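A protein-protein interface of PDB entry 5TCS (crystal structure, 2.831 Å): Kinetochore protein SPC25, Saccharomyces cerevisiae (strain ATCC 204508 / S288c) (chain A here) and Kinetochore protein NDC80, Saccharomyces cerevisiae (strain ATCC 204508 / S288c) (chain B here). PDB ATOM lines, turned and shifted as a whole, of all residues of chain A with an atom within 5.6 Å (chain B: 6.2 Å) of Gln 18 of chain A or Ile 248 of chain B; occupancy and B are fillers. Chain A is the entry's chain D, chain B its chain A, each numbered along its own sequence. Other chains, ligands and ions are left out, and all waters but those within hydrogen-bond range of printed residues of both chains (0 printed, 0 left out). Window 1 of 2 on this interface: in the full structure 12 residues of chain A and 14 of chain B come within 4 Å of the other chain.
The side-chain amide nitrogen of Gln 18 of chain A sits close to the side-chain amide oxygen of Asn 247 of chain B (3.2 Å).
Phe 244 of chain B touches Met 14 of chain A. Phe 17 of chain A touches Phe 244 of chain B. CD2 of Phe 17 of chain A touches CD1 of Ile 248 of chain B, at 3.7 Å. Gln 18 of chain A touches Phe 244 of chain B (NE2 to CA, 3.9 Å). Gln 18 of chain A touches Ile 248 of chain B.
Printed residues of chain A that touch a printed residue of chain B: Met 14, Phe 17 and Gln 18. Hydrophobic or aromatic side chains of chain A that line the printed part of chain B: Met 14 and Phe 17. Among the printed residues, no Asp or Glu carboxylate lies within 4 Å of a Lys or Arg side-chain nitrogen of the other chain.
Gly 16 of chain A touches none of the printed residues of chain B. Of the printed residues of chain B, Phe 17 of chain A touches Phe 244 (3.5 Å) and Ile 248 (3.7 Å). Of chain B, only Phe 244 (3.9 Å), Asn 247 (2.9 Å) and Ile 248 (3.8 Å) come within 4 Å of Gln 18 of chain A. Val 21 of chain A touches none of the printed residues of chain B. Of the printed residues of chain A, Phe 244 of chain B touches Met 14 (3.3 Å), Phe 17 (3.5 Å) and Gln 18 (3.9 Å). The nearest printed residue of chain B that does not touch Met 14 of chain A is Lys 245 of chain B (5.7 Å).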
ATOM      1  N   ARG A  13      -7.590 -27.977 -33.302  1.00  0.00           N
ATOM      2  CA  ARG A  13      -6.683 -27.088 -32.583  1.00  0.00           C
ATOM      3  C   ARG A  13      -7.379 -25.789 -32.201  1.00  0.00           C
ATOM      4  O   ARG A  13      -7.299 -25.341 -31.050  1.00  0.00           O
ATOM      5  CB  ARG A  13      -5.442 -26.795 -33.430  1.00  0.00           C
ATOM      6  CG  ARG A  13      -4.529 -27.990 -33.641  1.00  0.00           C
ATOM      7  CD  ARG A  13      -3.077 -27.548 -33.753  1.00  0.00           C
ATOM      8  NE  ARG A  13      -2.227 -28.589 -34.333  1.00  0.00           N
ATOM      9  CZ  ARG A  13      -1.587 -28.503 -35.498  1.00  0.00           C
ATOM     10  NH1 ARG A  13      -1.667 -27.409 -36.247  1.00  0.00           N
ATOM     11  NH2 ARG A  13      -0.845 -29.521 -35.916  1.00  0.00           N
ATOM     12  N   MET A  14      -8.074 -25.178 -33.152  1.00  0.00           N
ATOM     13  CA  MET A  14      -8.790 -23.938 -32.895  1.00  0.00           C
ATOM     14  C   MET A  14      -9.754 -24.113 -31.727  1.00  0.00           C
ATOM     15  O   MET A  14      -9.712 -23.343 -30.766  1.00  0.00           O
ATOM     16  CB  MET A  14      -9.531 -23.482 -34.153  1.00  0.00           C
ATOM     17  CG  MET A  14      -8.618 -22.774 -35.144  1.00  0.00           C
ATOM     18  SD  MET A  14      -9.292 -22.714 -36.967  1.00  0.00           S
ATOM     19  CE  MET A  14     -10.423 -21.148 -36.847  1.00  0.00           C
ATOM     20  N   ASP A  15     -10.599 -25.146 -31.789  1.00  0.00           N
ATOM     21  CA  ASP A  15     -11.524 -25.392 -30.688  1.00  0.00           C
ATOM     22  C   ASP A  15     -10.782 -25.522 -29.365  1.00  0.00           C
ATOM     23  O   ASP A  15     -11.298 -25.109 -28.321  1.00  0.00           O
ATOM     24  CB  ASP A  15     -12.353 -26.646 -30.960  1.00  0.00           C
ATOM     25  CG  ASP A  15     -13.369 -26.443 -32.069  1.00  0.00           C
ATOM     26  OD1 ASP A  15     -13.723 -25.277 -32.343  1.00  0.00           O
ATOM     27  OD2 ASP A  15     -13.817 -27.449 -32.661  1.00  0.00           O
ATOM     28  N   GLY A  16      -9.573 -26.085 -29.388  1.00  0.00           N
ATOM     29  CA  GLY A  16      -8.768 -26.123 -28.179  1.00  0.00           C
ATOM     30  C   GLY A  16      -8.269 -24.745 -27.787  1.00  0.00           C
ATOM     31  O   GLY A  16      -8.399 -24.328 -26.634  1.00  0.00           O
ATOM     32  N   PHE A  17      -7.700 -24.016 -28.749  1.00  0.00           N
ATOM     33  CA  PHE A  17      -7.243 -22.658 -28.484  1.00  0.00           C
ATOM     34  C   PHE A  17      -8.383 -21.824 -27.917  1.00  0.00           C
ATOM     35  O   PHE A  17      -8.298 -21.289 -26.805  1.00  0.00           O
ATOM     36  CB  PHE A  17      -6.695 -22.042 -29.773  1.00  0.00           C
ATOM     37  CG  PHE A  17      -5.898 -20.790 -29.560  1.00  0.00           C
ATOM     38  CD1 PHE A  17      -4.574 -20.859 -29.160  1.00  0.00           C
ATOM     39  CD2 PHE A  17      -6.468 -19.546 -29.767  1.00  0.00           C
ATOM     40  CE1 PHE A  17      -3.837 -19.711 -28.965  1.00  0.00           C
ATOM     41  CE2 PHE A  17      -5.735 -18.394 -29.574  1.00  0.00           C
ATOM     42  CZ  PHE A  17      -4.416 -18.477 -29.173  1.00  0.00           C
ATOM     43  N   GLN A  18      -9.475 -21.731 -28.676  1.00  0.00           N
ATOM     44  CA  GLN A  18     -10.709 -21.103 -28.221  1.00  0.00           C
ATOM     45  C   GLN A  18     -10.993 -21.441 -26.763  1.00  0.00           C
ATOM     46  O   GLN A  18     -11.371 -20.568 -25.975  1.00  0.00           O
ATOM     47  CB  GLN A  18     -11.864 -21.568 -29.106  1.00  0.00           C
ATOM     48  CG  GLN A  18     -12.980 -20.565 -29.287  1.00  0.00           C
ATOM     49  CD  GLN A  18     -14.035 -21.046 -30.268  1.00  0.00           C
ATOM     50  OE1 GLN A  18     -14.315 -22.242 -30.355  1.00  0.00           O
ATOM     51  NE2 GLN A  18     -14.618 -20.117 -31.017  1.00  0.00           N
ATOM     52  N   LYS A  19     -10.802 -22.709 -26.396  1.00  0.00           N
ATOM     53  CA  LYS A  19     -11.009 -23.132 -25.017  1.00  0.00           C
ATOM     54  C   LYS A  19      -9.905 -22.595 -24.114  1.00  0.00           C
ATOM     55  O   LYS A  19     -10.169 -21.854 -23.158  1.00  0.00           O
ATOM     56  CB  LYS A  19     -11.073 -24.661 -24.961  1.00  0.00           C
ATOM     57  CG  LYS A  19     -11.225 -25.258 -23.576  1.00  0.00           C
ATOM     58  CD  LYS A  19     -11.353 -26.776 -23.662  1.00  0.00           C
ATOM     59  CE  LYS A  19     -11.893 -27.382 -22.378  1.00  0.00           C
ATOM     60  NZ  LYS A  19     -12.118 -28.848 -22.517  1.00  0.00           N
ATOM     61  N   ASP A  20      -8.651 -22.934 -24.425  1.00  0.00           N
ATOM     62  CA  ASP A  20      -7.536 -22.588 -23.550  1.00  0.00           C
ATOM     63  C   ASP A  20      -7.535 -21.101 -23.216  1.00  0.00           C
ATOM     64  O   ASP A  20      -7.486 -20.716 -22.042  1.00  0.00           O
ATOM     65  CB  ASP A  20      -6.215 -22.994 -24.206  1.00  0.00           C
ATOM     66  CG  ASP A  20      -6.087 -24.496 -24.375  1.00  0.00           C
ATOM     67  OD1 ASP A  20      -6.627 -25.239 -23.527  1.00  0.00           O
ATOM     68  OD2 ASP A  20      -5.451 -24.934 -25.357  1.00  0.00           O
ATOM     69  N   VAL A  21      -7.587 -20.248 -24.242  1.00  0.00           N
ATOM     70  CA  VAL A  21      -7.684 -18.805 -24.021  1.00  0.00           C
ATOM     71  C   VAL A  21      -8.759 -18.509 -22.983  1.00  0.00           C
ATOM     72  O   VAL A  21      -8.494 -17.913 -21.931  1.00  0.00           O
ATOM     73  CB  VAL A  21      -7.969 -18.077 -25.345  1.00  0.00           C
ATOM     74  CG1 VAL A  21      -8.370 -16.622 -25.097  1.00  0.00           C
ATOM     75  CG2 VAL A  21      -6.754 -18.142 -26.254  1.00  0.00           C
ATOM     76  N   ALA A  22      -9.991 -18.944 -23.263  1.00  0.00           N
ATOM     77  CA  ALA A  22     -11.109 -18.642 -22.375  1.00  0.00           C
ATOM     78  C   ALA A  22     -10.814 -19.049 -20.940  1.00  0.00           C
ATOM     79  O   ALA A  22     -11.289 -18.399 -19.999  1.00  0.00           O
ATOM     80  CB  ALA A  22     -12.373 -19.344 -22.871  1.00  0.00           C
ATOM     81  N   GLN A  23     -10.027 -20.109 -20.746  1.00  0.00           N
ATOM     82  CA  GLN A  23      -9.762 -20.595 -19.400  1.00  0.00           C
ATOM     83  C   GLN A  23      -8.759 -19.709 -18.670  1.00  0.00           C
ATOM     84  O   GLN A  23      -8.884 -19.497 -17.458  1.00  0.00           O
ATOM     85  CB  GLN A  23      -9.255 -22.037 -19.462  1.00  0.00           C
ATOM     86  CG  GLN A  23      -9.690 -22.893 -18.287  1.00  0.00           C
ATOM     87  CD  GLN A  23      -9.230 -24.333 -18.413  1.00  0.00           C
ATOM     88  OE1 GLN A  23      -9.320 -24.936 -19.484  1.00  0.00           O
ATOM     89  NE2 GLN A  23      -8.731 -24.891 -17.316  1.00  0.00           N
ATOM     90  N   LYS B 243     -15.851 -16.795 -37.048  1.00  0.00           N
ATOM     91  CA  LYS B 243     -16.349 -17.033 -35.700  1.00  0.00           C
ATOM     92  C   LYS B 243     -15.194 -17.123 -34.715  1.00  0.00           C
ATOM     93  O   LYS B 243     -15.116 -16.352 -33.749  1.00  0.00           O
ATOM     94  CB  LYS B 243     -17.188 -18.314 -35.658  1.00  0.00           C
ATOM     95  CG  LYS B 243     -18.582 -18.183 -36.240  1.00  0.00           C
ATOM     96  CD  LYS B 243     -19.438 -19.368 -35.822  1.00  0.00           C
ATOM     97  CE  LYS B 243     -20.657 -19.544 -36.714  1.00  0.00           C
ATOM     98  NZ  LYS B 243     -21.005 -20.984 -36.869  1.00  0.00           N
ATOM     99  N   PHE B 244     -14.262 -18.040 -34.983  1.00  0.00           N
ATOM    100  CA  PHE B 244     -13.115 -18.232 -34.106  1.00  0.00           C
ATOM    101  C   PHE B 244     -12.536 -16.887 -33.690  1.00  0.00           C
ATOM    102  O   PHE B 244     -12.570 -16.519 -32.508  1.00  0.00           O
ATOM    103  CB  PHE B 244     -12.064 -19.098 -34.814  1.00  0.00           C
ATOM    104  CG  PHE B 244     -10.747 -19.174 -34.094  1.00  0.00           C
ATOM    105  CD1 PHE B 244     -10.633 -19.860 -32.897  1.00  0.00           C
ATOM    106  CD2 PHE B 244      -9.617 -18.576 -34.627  1.00  0.00           C
ATOM    107  CE1 PHE B 244      -9.421 -19.935 -32.239  1.00  0.00           C
ATOM    108  CE2 PHE B 244      -8.403 -18.650 -33.976  1.00  0.00           C
ATOM    109  CZ  PHE B 244      -8.306 -19.332 -32.779  1.00  0.00           C
ATOM    110  N   LYS B 245     -12.062 -16.114 -34.670  1.00  0.00           N
ATOM    111  CA  LYS B 245     -11.468 -14.816 -34.379  1.00  0.00           C
ATOM    112  C   LYS B 245     -12.370 -14.020 -33.443  1.00  0.00           C
ATOM    113  O   LYS B 245     -11.966 -13.641 -32.340  1.00  0.00           O
ATOM    114  CB  LYS B 245     -11.228 -14.060 -35.687  1.00  0.00           C
ATOM    115  CG  LYS B 245     -10.591 -12.694 -35.524  1.00  0.00           C
ATOM    116  CD  LYS B 245      -9.230 -12.784 -34.855  1.00  0.00           C
ATOM    117  CE  LYS B 245      -8.505 -11.454 -34.930  1.00  0.00           C
ATOM    118  NZ  LYS B 245      -7.321 -11.430 -34.045  1.00  0.00           N
ATOM    119  N   ILE B 246     -13.620 -13.809 -33.854  1.00  0.00           N
ATOM    120  CA  ILE B 246     -14.608 -13.052 -33.089  1.00  0.00           C
ATOM    121  C   ILE B 246     -14.524 -13.542 -31.649  1.00  0.00           C
ATOM    122  O   ILE B 246     -14.219 -12.762 -30.736  1.00  0.00           O
ATOM    123  CB  ILE B 246     -16.033 -13.211 -33.673  1.00  0.00           C
ATOM    124  CG1 ILE B 246     -16.276 -12.168 -34.769  1.00  0.00           C
ATOM    125  CG2 ILE B 246     -17.100 -13.057 -32.584  1.00  0.00           C
ATOM    126  CD1 ILE B 246     -15.191 -12.100 -35.836  1.00  0.00           C
ATOM    127  N   ASN B 247     -14.748 -14.840 -31.452  1.00  0.00           N
ATOM    128  CA  ASN B 247     -14.788 -15.372 -30.098  1.00  0.00           C
ATOM    129  C   ASN B 247     -13.548 -14.951 -29.322  1.00  0.00           C
ATOM    130  O   ASN B 247     -13.649 -14.352 -28.245  1.00  0.00           O
ATOM    131  CB  ASN B 247     -14.925 -16.895 -30.126  1.00  0.00           C
ATOM    132  CG  ASN B 247     -15.215 -17.481 -28.755  1.00  0.00           C
ATOM    133  OD1 ASN B 247     -14.510 -18.373 -28.289  1.00  0.00           O
ATOM    134  ND2 ASN B 247     -16.250 -16.967 -28.095  1.00  0.00           N
ATOM    135  N   ILE B 248     -12.361 -15.219 -29.877  1.00  0.00           N
ATOM    136  CA  ILE B 248     -11.128 -14.872 -29.175  1.00  0.00           C
ATOM    137  C   ILE B 248     -11.161 -13.406 -28.773  1.00  0.00           C
ATOM    138  O   ILE B 248     -10.937 -13.053 -27.609  1.00  0.00           O
ATOM    139  CB  ILE B 248      -9.894 -15.177 -30.044  1.00  0.00           C
ATOM    140  CG1 ILE B 248      -9.877 -16.640 -30.505  1.00  0.00           C
ATOM    141  CG2 ILE B 248      -8.623 -14.838 -29.268  1.00  0.00           C
ATOM    142  CD1 ILE B 248      -9.607 -17.648 -29.405  1.00  0.00           C
ATOM    143  N   GLN B 249     -11.462 -12.530 -29.734  1.00  0.00           N
ATOM    144  CA  GLN B 249     -11.470 -11.104 -29.441  1.00  0.00           C
ATOM    145  C   GLN B 249     -12.402 -10.804 -28.276  1.00  0.00           C
ATOM    146  O   GLN B 249     -12.035 -10.066 -27.353  1.00  0.00           O
ATOM    147  CB  GLN B 249     -11.867 -10.312 -30.687  1.00  0.00           C
ATOM    148  CG  GLN B 249     -11.018 -10.648 -31.910  1.00  0.00           C
ATOM    149  CD  GLN B 249     -10.561  -9.422 -32.678  1.00  0.00           C
ATOM    150  OE1 GLN B 249      -9.364  -9.144 -32.772  1.00  0.00           O
ATOM    151  NE2 GLN B 249     -11.513  -8.687 -33.245  1.00  0.00           N
ATOM    152  N   SER B 250     -13.595 -11.402 -28.279  1.00  0.00           N
ATOM    153  CA  SER B 250     -14.499 -11.247 -27.148  1.00  0.00           C
ATOM    154  C   SER B 250     -13.777 -11.571 -25.847  1.00  0.00           C
ATOM    155  O   SER B 250     -13.696 -10.738 -24.936  1.00  0.00           O
ATOM    156  CB  SER B 250     -15.726 -12.142 -27.334  1.00  0.00           C
ATOM    157  OG  SER B 250     -16.609 -12.034 -26.229  1.00  0.00           O
ATOM    158  N   SER B 251     -13.205 -12.778 -25.765  1.00  0.00           N
ATOM    159  CA  SER B 251     -12.489 -13.184 -24.562  1.00  0.00           C
ATOM    160  C   SER B 251     -11.493 -12.119 -24.127  1.00  0.00           C
ATOM    161  O   SER B 251     -11.340 -11.852 -22.928  1.00  0.00           O
ATOM    162  CB  SER B 251     -11.774 -14.514 -24.801  1.00  0.00           C
ATOM    163  OG  SER B 251     -12.694 -15.591 -24.830  1.00  0.00           O
ATOM    164  N   LEU B 252     -10.810 -11.493 -25.086  1.00  0.00           N
ATOM    165  CA  LEU B 252      -9.858 -10.444 -24.741  1.00  0.00           C
ATOM    166  C   LEU B 252     -10.582  -9.205 -24.235  1.00  0.00           C
ATOM    167  O   LEU B 252     -10.288  -8.702 -23.143  1.00  0.00           O
ATOM    168  CB  LEU B 252      -8.990 -10.104 -25.953  1.00  0.00           C
ATOM    169  CG  LEU B 252      -8.085 -11.222 -26.481  1.00  0.00           C
ATOM    170  CD1 LEU B 252      -7.469 -10.822 -27.810  1.00  0.00           C
ATOM    171  CD2 LEU B 252      -6.997 -11.565 -25.476  1.00  0.00           C
ATOM    172  N   GLU B 253     -11.558  -8.714 -25.004  1.00  0.00           N
ATOM    173  CA  GLU B 253     -12.213  -7.457 -24.661  1.00  0.00           C
ATOM    174  C   GLU B 253     -12.773  -7.505 -23.245  1.00  0.00           C
ATOM    175  O   GLU B 253     -12.610  -6.558 -22.467  1.00  0.00           O
ATOM    176  CB  GLU B 253     -13.319  -7.154 -25.669  1.00  0.00           C
ATOM    177  CG  GLU B 253     -13.846  -5.737 -25.585  1.00  0.00           C
ATOM    178  CD  GLU B 253     -14.862  -5.429 -26.666  1.00  0.00           C
ATOM    179  OE1 GLU B 253     -15.653  -6.332 -27.017  1.00  0.00           O
ATOM    180  OE2 GLU B 253     -14.867  -4.286 -27.171  1.00  0.00           O
